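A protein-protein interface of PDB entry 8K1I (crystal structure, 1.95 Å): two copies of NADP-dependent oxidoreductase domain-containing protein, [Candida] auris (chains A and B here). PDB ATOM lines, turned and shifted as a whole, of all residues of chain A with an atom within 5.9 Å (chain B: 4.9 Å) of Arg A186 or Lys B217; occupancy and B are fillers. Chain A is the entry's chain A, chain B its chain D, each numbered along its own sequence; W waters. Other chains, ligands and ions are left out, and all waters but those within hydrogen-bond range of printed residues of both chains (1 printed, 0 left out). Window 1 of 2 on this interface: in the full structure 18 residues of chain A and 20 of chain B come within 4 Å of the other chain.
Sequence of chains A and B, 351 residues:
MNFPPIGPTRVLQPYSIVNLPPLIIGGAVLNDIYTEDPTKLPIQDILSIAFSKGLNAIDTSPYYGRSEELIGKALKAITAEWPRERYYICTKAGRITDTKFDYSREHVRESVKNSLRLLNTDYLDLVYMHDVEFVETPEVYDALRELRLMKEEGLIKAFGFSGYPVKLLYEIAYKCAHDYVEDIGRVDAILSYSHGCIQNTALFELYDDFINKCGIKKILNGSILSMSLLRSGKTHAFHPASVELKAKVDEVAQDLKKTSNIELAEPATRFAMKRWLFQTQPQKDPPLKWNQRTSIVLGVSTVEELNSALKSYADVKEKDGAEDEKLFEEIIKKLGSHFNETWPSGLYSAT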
ATOM      1  N   LYS A 151     -10.446  23.054  -3.906  1.00  0.00           N
ATOM      2  CA  LYS A 151     -10.428  22.419  -2.590  1.00  0.00           C
ATOM      3  C   LYS A 151     -11.830  22.363  -2.005  1.00  0.00           C
ATOM      4  O   LYS A 151     -12.259  21.314  -1.520  1.00  0.00           O
ATOM      5  CB  LYS A 151      -9.477  23.166  -1.652  1.00  0.00           C
ATOM      6  CG  LYS A 151      -9.396  22.574  -0.262  1.00  0.00           C
ATOM      7  CD  LYS A 151      -8.252  23.218   0.587  1.00  0.00           C
ATOM      8  CE  LYS A 151      -8.551  23.073   2.083  1.00  0.00           C
ATOM      9  NZ  LYS A 151      -7.477  23.769   2.889  1.00  0.00           N
ATOM     10  N   PHE A 159      -3.986  23.071  -1.056  1.00  0.00           N
ATOM     11  CA  PHE A 159      -3.475  23.936  -2.110  1.00  0.00           C
ATOM     12  C   PHE A 159      -2.356  24.803  -1.551  1.00  0.00           C
ATOM     13  O   PHE A 159      -2.197  24.958  -0.340  1.00  0.00           O
ATOM     14  CB  PHE A 159      -4.577  24.842  -2.713  1.00  0.00           C
ATOM     15  CG  PHE A 159      -4.948  26.033  -1.843  1.00  0.00           C
ATOM     16  CD1 PHE A 159      -5.595  25.863  -0.621  1.00  0.00           C
ATOM     17  CD2 PHE A 159      -4.684  27.323  -2.274  1.00  0.00           C
ATOM     18  CE1 PHE A 159      -5.915  26.953   0.167  1.00  0.00           C
ATOM     19  CE2 PHE A 159      -5.029  28.402  -1.516  1.00  0.00           C
ATOM     20  CZ  PHE A 159      -5.642  28.225  -0.287  1.00  0.00           C
ATOM     21  N   ALA A 173       2.065  34.336   0.965  1.00  0.00           N
ATOM     22  CA  ALA A 173       1.358  33.560   1.978  1.00  0.00           C
ATOM     23  C   ALA A 173       0.760  34.473   3.045  1.00  0.00           C
ATOM     24  O   ALA A 173      -0.356  34.234   3.528  1.00  0.00           O
ATOM     25  CB  ALA A 173       2.297  32.533   2.606  1.00  0.00           C
ATOM     26  N   CYS A 176      -2.429  36.102   1.839  1.00  0.00           N
ATOM     27  CA  CYS A 176      -3.589  35.207   1.769  1.00  0.00           C
ATOM     28  C   CYS A 176      -4.243  35.032   3.121  1.00  0.00           C
ATOM     29  O   CYS A 176      -5.470  34.840   3.209  1.00  0.00           O
ATOM     30  CB  CYS A 176      -3.191  33.822   1.240  1.00  0.00           C
ATOM     31  SG  CYS A 176      -2.637  33.793  -0.440  1.00  0.00           S
ATOM     32  N   ALA A 177      -3.439  35.063   4.174  1.00  0.00           N
ATOM     33  CA  ALA A 177      -3.896  34.887   5.536  1.00  0.00           C
ATOM     34  C   ALA A 177      -4.369  36.181   6.165  1.00  0.00           C
ATOM     35  O   ALA A 177      -4.836  36.156   7.308  1.00  0.00           O
ATOM     36  CB  ALA A 177      -2.773  34.294   6.394  1.00  0.00           C
ATOM     37  N   VAL A 181      -8.184  37.044   3.449  1.00  0.00           N
ATOM     38  CA  VAL A 181      -8.591  35.944   4.303  1.00  0.00           C
ATOM     39  C   VAL A 181      -9.953  35.412   3.890  1.00  0.00           C
ATOM     40  O   VAL A 181     -10.183  34.200   3.902  1.00  0.00           O
ATOM     41  CB  VAL A 181      -8.568  36.376   5.778  1.00  0.00           C
ATOM     42  CG1 VAL A 181      -9.425  37.594   6.004  1.00  0.00           C
ATOM     43  CG2 VAL A 181      -9.007  35.228   6.636  1.00  0.00           C
ATOM     44  N   ILE A 184      -9.319  33.744   0.174  1.00  0.00           N
ATOM     45  CA  ILE A 184      -8.291  32.706   0.073  1.00  0.00           C
ATOM     46  C   ILE A 184      -8.008  32.059   1.426  1.00  0.00           C
ATOM     47  O   ILE A 184      -8.208  30.851   1.604  1.00  0.00           O
ATOM     48  CB  ILE A 184      -6.990  33.271  -0.536  1.00  0.00           C
ATOM     49  CG1 ILE A 184      -7.292  34.107  -1.784  1.00  0.00           C
ATOM     50  CG2 ILE A 184      -5.987  32.137  -0.866  1.00  0.00           C
ATOM     51  CD1 ILE A 184      -6.018  34.561  -2.536  1.00  0.00           C
ATOM     52  N   GLY A 185      -7.555  32.853   2.402  1.00  0.00           N
ATOM     53  CA  GLY A 185      -7.135  32.289   3.672  1.00  0.00           C
ATOM     54  C   GLY A 185      -5.774  31.625   3.549  1.00  0.00           C
ATOM     55  O   GLY A 185      -5.179  31.524   2.466  1.00  0.00           O
ATOM     56  N   ARG A 186      -5.275  31.169   4.699  1.00  0.00           N
ATOM     57  CA  ARG A 186      -3.965  30.505   4.765  1.00  0.00           C
ATOM     58  C   ARG A 186      -3.849  29.433   3.691  1.00  0.00           C
ATOM     59  O   ARG A 186      -4.770  28.633   3.494  1.00  0.00           O
ATOM     60  CB  ARG A 186      -3.764  29.890   6.159  1.00  0.00           C
ATOM     61  CG  ARG A 186      -4.531  30.682   7.245  1.00  0.00           C
ATOM     62  CD  ARG A 186      -3.875  30.782   8.625  1.00  0.00           C
ATOM     63  NE  ARG A 186      -4.520  29.919   9.589  1.00  0.00           N
ATOM     64  CZ  ARG A 186      -4.646  30.138  10.891  1.00  0.00           C
ATOM     65  NH1 ARG A 186      -4.208  31.249  11.466  1.00  0.00           N
ATOM     66  NH2 ARG A 186      -5.208  29.200  11.645  1.00  0.00           N
ATOM     67  N   VAL A 187      -2.722  29.431   2.972  1.00  0.00           N
ATOM     68  CA  VAL A 187      -2.451  28.298   2.098  1.00  0.00           C
ATOM     69  C   VAL A 187      -2.079  27.096   2.951  1.00  0.00           C
ATOM     70  O   VAL A 187      -1.553  27.229   4.065  1.00  0.00           O
ATOM     71  CB  VAL A 187      -1.342  28.602   1.071  1.00  0.00           C
ATOM     72  CG1 VAL A 187      -1.757  29.768   0.155  1.00  0.00           C
ATOM     73  CG2 VAL A 187      -0.001  28.832   1.741  1.00  0.00           C
ATOM     74  N   ASP A 188      -2.333  25.902   2.423  1.00  0.00           N
ATOM     75  CA  ASP A 188      -1.930  24.704   3.147  1.00  0.00           C
ATOM     76  C   ASP A 188      -0.422  24.539   3.147  1.00  0.00           C
ATOM     77  O   ASP A 188       0.152  24.033   4.117  1.00  0.00           O
ATOM     78  CB  ASP A 188      -2.583  23.459   2.540  1.00  0.00           C
ATOM     79  CG  ASP A 188      -4.092  23.511   2.559  1.00  0.00           C
ATOM     80  OD1 ASP A 188      -4.662  23.414   3.666  1.00  0.00           O
ATOM     81  OD2 ASP A 188      -4.723  23.597   1.484  1.00  0.00           O
ATOM     82  N   CYS A 214       2.190  33.438   8.754  1.00  0.00           N
ATOM     83  CA  CYS A 214       1.399  33.140   7.565  1.00  0.00           C
ATOM     84  C   CYS A 214       0.402  32.001   7.765  1.00  0.00           C
ATOM     85  O   CYS A 214      -0.475  31.793   6.903  1.00  0.00           O
ATOM     86  CB  CYS A 214       2.321  32.763   6.404  1.00  0.00           C
ATOM     87  SG  CYS A 214       3.436  34.067   5.865  1.00  0.00           S
ATOM     88  N   GLY A 215       0.541  31.232   8.841  1.00  0.00           N
ATOM     89  CA  GLY A 215      -0.399  30.152   9.129  1.00  0.00           C
ATOM     90  C   GLY A 215      -0.308  28.923   8.242  1.00  0.00           C
ATOM     91  O   GLY A 215      -1.267  28.123   8.190  1.00  0.00           O
ATOM     92  N   ILE A 216       0.809  28.753   7.525  1.00  0.00           N
ATOM     93  CA  ILE A 216       1.003  27.584   6.677  1.00  0.00           C
ATOM     94  C   ILE A 216       1.121  26.337   7.538  1.00  0.00           C
ATOM     95  O   ILE A 216       1.819  26.340   8.555  1.00  0.00           O
ATOM     96  CB  ILE A 216       2.260  27.773   5.805  1.00  0.00           C
ATOM     97  CG1 ILE A 216       2.085  28.978   4.874  1.00  0.00           C
ATOM     98  CG2 ILE A 216       2.637  26.491   5.111  1.00  0.00           C
ATOM     99  CD1 ILE A 216       3.371  29.646   4.528  1.00  0.00           C
ATOM    100  N   VAL B  18     -13.900  31.651   9.614  1.00  0.00           N
ATOM    101  CA  VAL B  18     -13.439  33.003   9.917  1.00  0.00           C
ATOM    102  C   VAL B  18     -14.510  34.020   9.530  1.00  0.00           C
ATOM    103  O   VAL B  18     -14.508  35.161  10.015  1.00  0.00           O
ATOM    104  CB  VAL B  18     -12.110  33.337   9.214  1.00  0.00           C
ATOM    105  CG1 VAL B  18     -11.125  32.179   9.405  1.00  0.00           C
ATOM    106  CG2 VAL B  18     -12.326  33.693   7.731  1.00  0.00           C
ATOM    107  N   LYS B 151     -15.835  16.494  12.212  1.00  0.00           N
ATOM    108  CA  LYS B 151     -15.490  17.464  11.180  1.00  0.00           C
ATOM    109  C   LYS B 151     -15.115  16.785   9.869  1.00  0.00           C
ATOM    110  O   LYS B 151     -15.543  17.216   8.790  1.00  0.00           O
ATOM    111  CB  LYS B 151     -14.340  18.354  11.661  1.00  0.00           C
ATOM    112  CG  LYS B 151     -14.182  19.603  10.823  1.00  0.00           C
ATOM    113  CD  LYS B 151     -13.095  20.561  11.376  1.00  0.00           C
ATOM    114  CE  LYS B 151     -12.531  21.414  10.219  1.00  0.00           C
ATOM    115  NZ  LYS B 151     -11.216  22.071  10.511  1.00  0.00           N
ATOM    116  N   ARG B 186      -4.430  21.771  14.498  1.00  0.00           N
ATOM    117  CA  ARG B 186      -4.834  23.051  15.097  1.00  0.00           C
ATOM    118  C   ARG B 186      -6.362  23.112  15.193  1.00  0.00           C
ATOM    119  O   ARG B 186      -7.077  22.587  14.333  1.00  0.00           O
ATOM    120  CB  ARG B 186      -4.262  24.250  14.312  1.00  0.00           C
ATOM    121  CG  ARG B 186      -2.883  23.954  13.670  1.00  0.00           C
ATOM    122  CD  ARG B 186      -1.979  25.167  13.414  1.00  0.00           C
ATOM    123  NE  ARG B 186      -2.250  25.705  12.096  1.00  0.00           N
ATOM    124  CZ  ARG B 186      -1.364  26.184  11.227  1.00  0.00           C
ATOM    125  NH1 ARG B 186      -0.075  26.313  11.514  1.00  0.00           N
ATOM    126  NH2 ARG B 186      -1.794  26.578  10.040  1.00  0.00           N
ATOM    127  N   VAL B 187      -6.868  23.664  16.297  1.00  0.00           N
ATOM    128  CA  VAL B 187      -8.318  23.822  16.443  1.00  0.00           C
ATOM    129  C   VAL B 187      -8.763  25.033  15.636  1.00  0.00           C
ATOM    130  O   VAL B 187      -7.991  25.977  15.392  1.00  0.00           O
ATOM    131  CB  VAL B 187      -8.769  23.940  17.920  1.00  0.00           C
ATOM    132  CG1 VAL B 187      -8.142  22.876  18.737  1.00  0.00           C
ATOM    133  CG2 VAL B 187      -8.482  25.343  18.502  1.00  0.00           C
ATOM    134  N   ASP B 188     -10.018  24.980  15.176  1.00  0.00           N
ATOM    135  CA  ASP B 188     -10.561  26.043  14.324  1.00  0.00           C
ATOM    136  C   ASP B 188     -10.849  27.330  15.100  1.00  0.00           C
ATOM    137  O   ASP B 188     -10.499  28.436  14.639  1.00  0.00           O
ATOM    138  CB  ASP B 188     -11.822  25.533  13.626  1.00  0.00           C
ATOM    139  CG  ASP B 188     -11.529  24.436  12.636  1.00  0.00           C
ATOM    140  OD1 ASP B 188     -10.732  24.689  11.696  1.00  0.00           O
ATOM    141  OD2 ASP B 188     -12.065  23.313  12.792  1.00  0.00           O
ATOM    142  N   ILE B 211      -3.377  32.967  17.747  1.00  0.00           N
ATOM    143  CA  ILE B 211      -3.383  32.924  16.285  1.00  0.00           C
ATOM    144  C   ILE B 211      -2.058  32.395  15.728  1.00  0.00           C
ATOM    145  O   ILE B 211      -2.045  31.523  14.849  1.00  0.00           O
ATOM    146  CB  ILE B 211      -3.697  34.317  15.723  1.00  0.00           C
ATOM    147  CG1 ILE B 211      -5.013  34.825  16.331  1.00  0.00           C
ATOM    148  CG2 ILE B 211      -3.658  34.294  14.167  1.00  0.00           C
ATOM    149  CD1 ILE B 211      -6.233  34.228  15.655  1.00  0.00           C
ATOM    150  N   GLY B 215      -1.921  28.540  15.821  1.00  0.00           N
ATOM    151  CA  GLY B 215      -2.566  28.448  14.517  1.00  0.00           C
ATOM    152  C   GLY B 215      -4.087  28.462  14.525  1.00  0.00           C
ATOM    153  O   GLY B 215      -4.700  28.022  13.544  1.00  0.00           O
ATOM    154  N   ILE B 216      -4.711  28.936  15.614  1.00  0.00           N
ATOM    155  CA  ILE B 216      -6.164  29.114  15.668  1.00  0.00           C
ATOM    156  C   ILE B 216      -6.633  30.081  14.592  1.00  0.00           C
ATOM    157  O   ILE B 216      -6.026  31.135  14.375  1.00  0.00           O
ATOM    158  CB  ILE B 216      -6.580  29.614  17.064  1.00  0.00           C
ATOM    159  CG1 ILE B 216      -6.155  28.613  18.150  1.00  0.00           C
ATOM    160  CG2 ILE B 216      -8.075  29.804  17.155  1.00  0.00           C
ATOM    161  CD1 ILE B 216      -6.509  29.025  19.587  1.00  0.00           C
ATOM    162  N   LYS B 217      -7.750  29.734  13.921  1.00  0.00           N
ATOM    163  CA  LYS B 217      -8.264  30.552  12.824  1.00  0.00           C
ATOM    164  C   LYS B 217      -9.095  31.752  13.295  1.00  0.00           C
ATOM    165  O   LYS B 217      -9.087  32.814  12.651  1.00  0.00           O
ATOM    166  CB  LYS B 217      -9.143  29.695  11.901  1.00  0.00           C
ATOM    167  CG  LYS B 217      -8.387  28.955  10.807  1.00  0.00           C
ATOM    168  CD  LYS B 217      -9.359  28.340   9.785  1.00  0.00           C
ATOM    169  CE  LYS B 217      -8.992  26.887   9.439  1.00  0.00           C
ATOM    170  NZ  LYS B 217     -10.181  26.071   9.018  1.00  0.00           N
ATOM    171  N   LYS B 218      -9.840  31.587  14.379  1.00  0.00           N
ATOM    172  CA  LYS B 218     -10.890  32.511  14.778  1.00  0.00           C
ATOM    173  C   LYS B 218     -10.997  32.438  16.293  1.00  0.00           C
ATOM    174  O   LYS B 218     -10.982  31.333  16.837  1.00  0.00           O
ATOM    175  CB  LYS B 218     -12.226  32.113  14.122  1.00  0.00           C
ATOM    176  CG  LYS B 218     -13.397  32.993  14.581  1.00  0.00           C
ATOM    177  CD  LYS B 218     -13.448  34.330  13.845  1.00  0.00           C
ATOM    178  CE  LYS B 218     -14.776  34.508  13.096  1.00  0.00           C
ATOM    179  NZ  LYS B 218     -15.031  35.939  12.758  1.00  0.00           N
ATOM    180  N   ILE B 219     -11.092  33.579  16.970  1.00  0.00           N
ATOM    181  CA  ILE B 219     -11.226  33.597  18.431  1.00  0.00           C
ATOM    182  C   ILE B 219     -12.446  34.414  18.812  1.00  0.00           C
ATOM    183  O   ILE B 219     -12.577  35.576  18.400  1.00  0.00           O
ATOM    184  CB  ILE B 219      -9.986  34.168  19.149  1.00  0.00           C
ATOM    185  CG1 ILE B 219      -8.698  33.513  18.647  1.00  0.00           C
ATOM    186  CG2 ILE B 219     -10.117  33.971  20.691  1.00  0.00           C
ATOM    187  CD1 ILE B 219      -7.451  34.316  19.016  1.00  0.00           C
ATOM    188  N   ARG B 293     -10.529  37.697  12.201  1.00  0.00           N
ATOM    189  CA  ARG B 293     -10.209  36.612  13.117  1.00  0.00           C
ATOM    190  C   ARG B 293     -10.918  36.755  14.467  1.00  0.00           C
ATOM    191  O   ARG B 293     -10.624  35.983  15.388  1.00  0.00           O
ATOM    192  CB  ARG B 293      -8.694  36.544  13.315  1.00  0.00           C
ATOM    193  CG  ARG B 293      -7.996  36.142  12.041  1.00  0.00           C
ATOM    194  CD  ARG B 293      -6.863  35.207  12.247  1.00  0.00           C
ATOM    195  NE  ARG B 293      -6.258  34.928  10.953  1.00  0.00           N
ATOM    196  CZ  ARG B 293      -6.654  33.963  10.133  1.00  0.00           C
ATOM    197  NH1 ARG B 293      -7.662  33.165  10.444  1.00  0.00           N
ATOM    198  NH2 ARG B 293      -5.997  33.770   8.988  1.00  0.00           N
HETATM  199  O   HOH W   1      -6.772  26.641  12.161  1.00  0.00           O
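The guanidinium group of Arg A186 sits close to the backbone carbonyl oxygen of Gly B215, 2.3 Å away.
The guanidinium group (NH2) of Arg B293 lies within hydrogen-bond range of the backbone carbonyl oxygen (O) of Ala A177, 3.1 Å away.
NH2 of Arg B186 is in hydrogen-bond range of O of Gly A215 (2.5 Å).
The backbone carbonyl oxygen (O) of Ile B216 sits at hydrogen-bond distance from the guanidinium group (NH1) of Arg A186, 3.4 Å away.
The guanidinium group (NH2) of Arg A186 sits close to the backbone NH (N) of Lys B217, at 3.5 Å.
Arg A186 touches Gly B215, and with the chains exchanged Gly A215 touches Arg B186.
Arg A186 touches Ile B216, and with the chains exchanged Ile A216 touches Arg B186.
Positions printed for both chains: 151, 186, 187, 188, 215 and 216.
Of the 8 pairs that touch across the chains among the printed residues, 4 have their exchanged pair printed and touching as well.
The backbone carbonyl oxygen of Arg B293 lies within hydrogen-bond range of the backbone NH of Ile B219 (2.9 Å).
O of Lys B217 lies within hydrogen-bond range of NH1 of Arg B293 (2.7 Å).
The backbone carbonyl oxygen (O) of Val B18 is in hydrogen-bond range of the side-chain amino group (NZ) of Lys B218, at 2.9 Å.
The side-chain carboxylate (OD1) of Asp B188 is in salt-bridge range of the side-chain amino group (NZ) of Lys B217 (3.1 Å).
Of the printed residues of chain B, Ala A177 touches Arg B293 (3.1 Å).
Ile A184 touches none of the printed residues of chain B.
Arg A186 touches four residues of chain B.
Of the printed residues of chain B, Gly A215 touches Arg B186.
Ile B211 touches none of the printed residues of chain A.
Of the printed residues of chain A, Lys B217 touches Arg A186.
The nearest residue of chain B that does not touch Arg A186 is Ile B211 (4.02 Å).
The nearest printed residue of chain B that does not touch Val A181 is Arg B293 (4.1 Å).
Hydrophobic or aromatic side chains of chain B that line the printed part of chain A: Val B18.
Among the printed residues, no Asp or Glu carboxylate lies within 4 Å of a Lys or Arg side-chain nitrogen of the other chain.
Water W1 bridges O of Gly B215 and NH2 of Arg A186.
CG2 of Val A181 touches CG2 of Val B18 (3.8 Å).
CD of Arg A186 touches NH2 of Arg B293 (3.7 Å).
Ile A216 touches Arg B186 (O to NH1, 3.5 Å).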
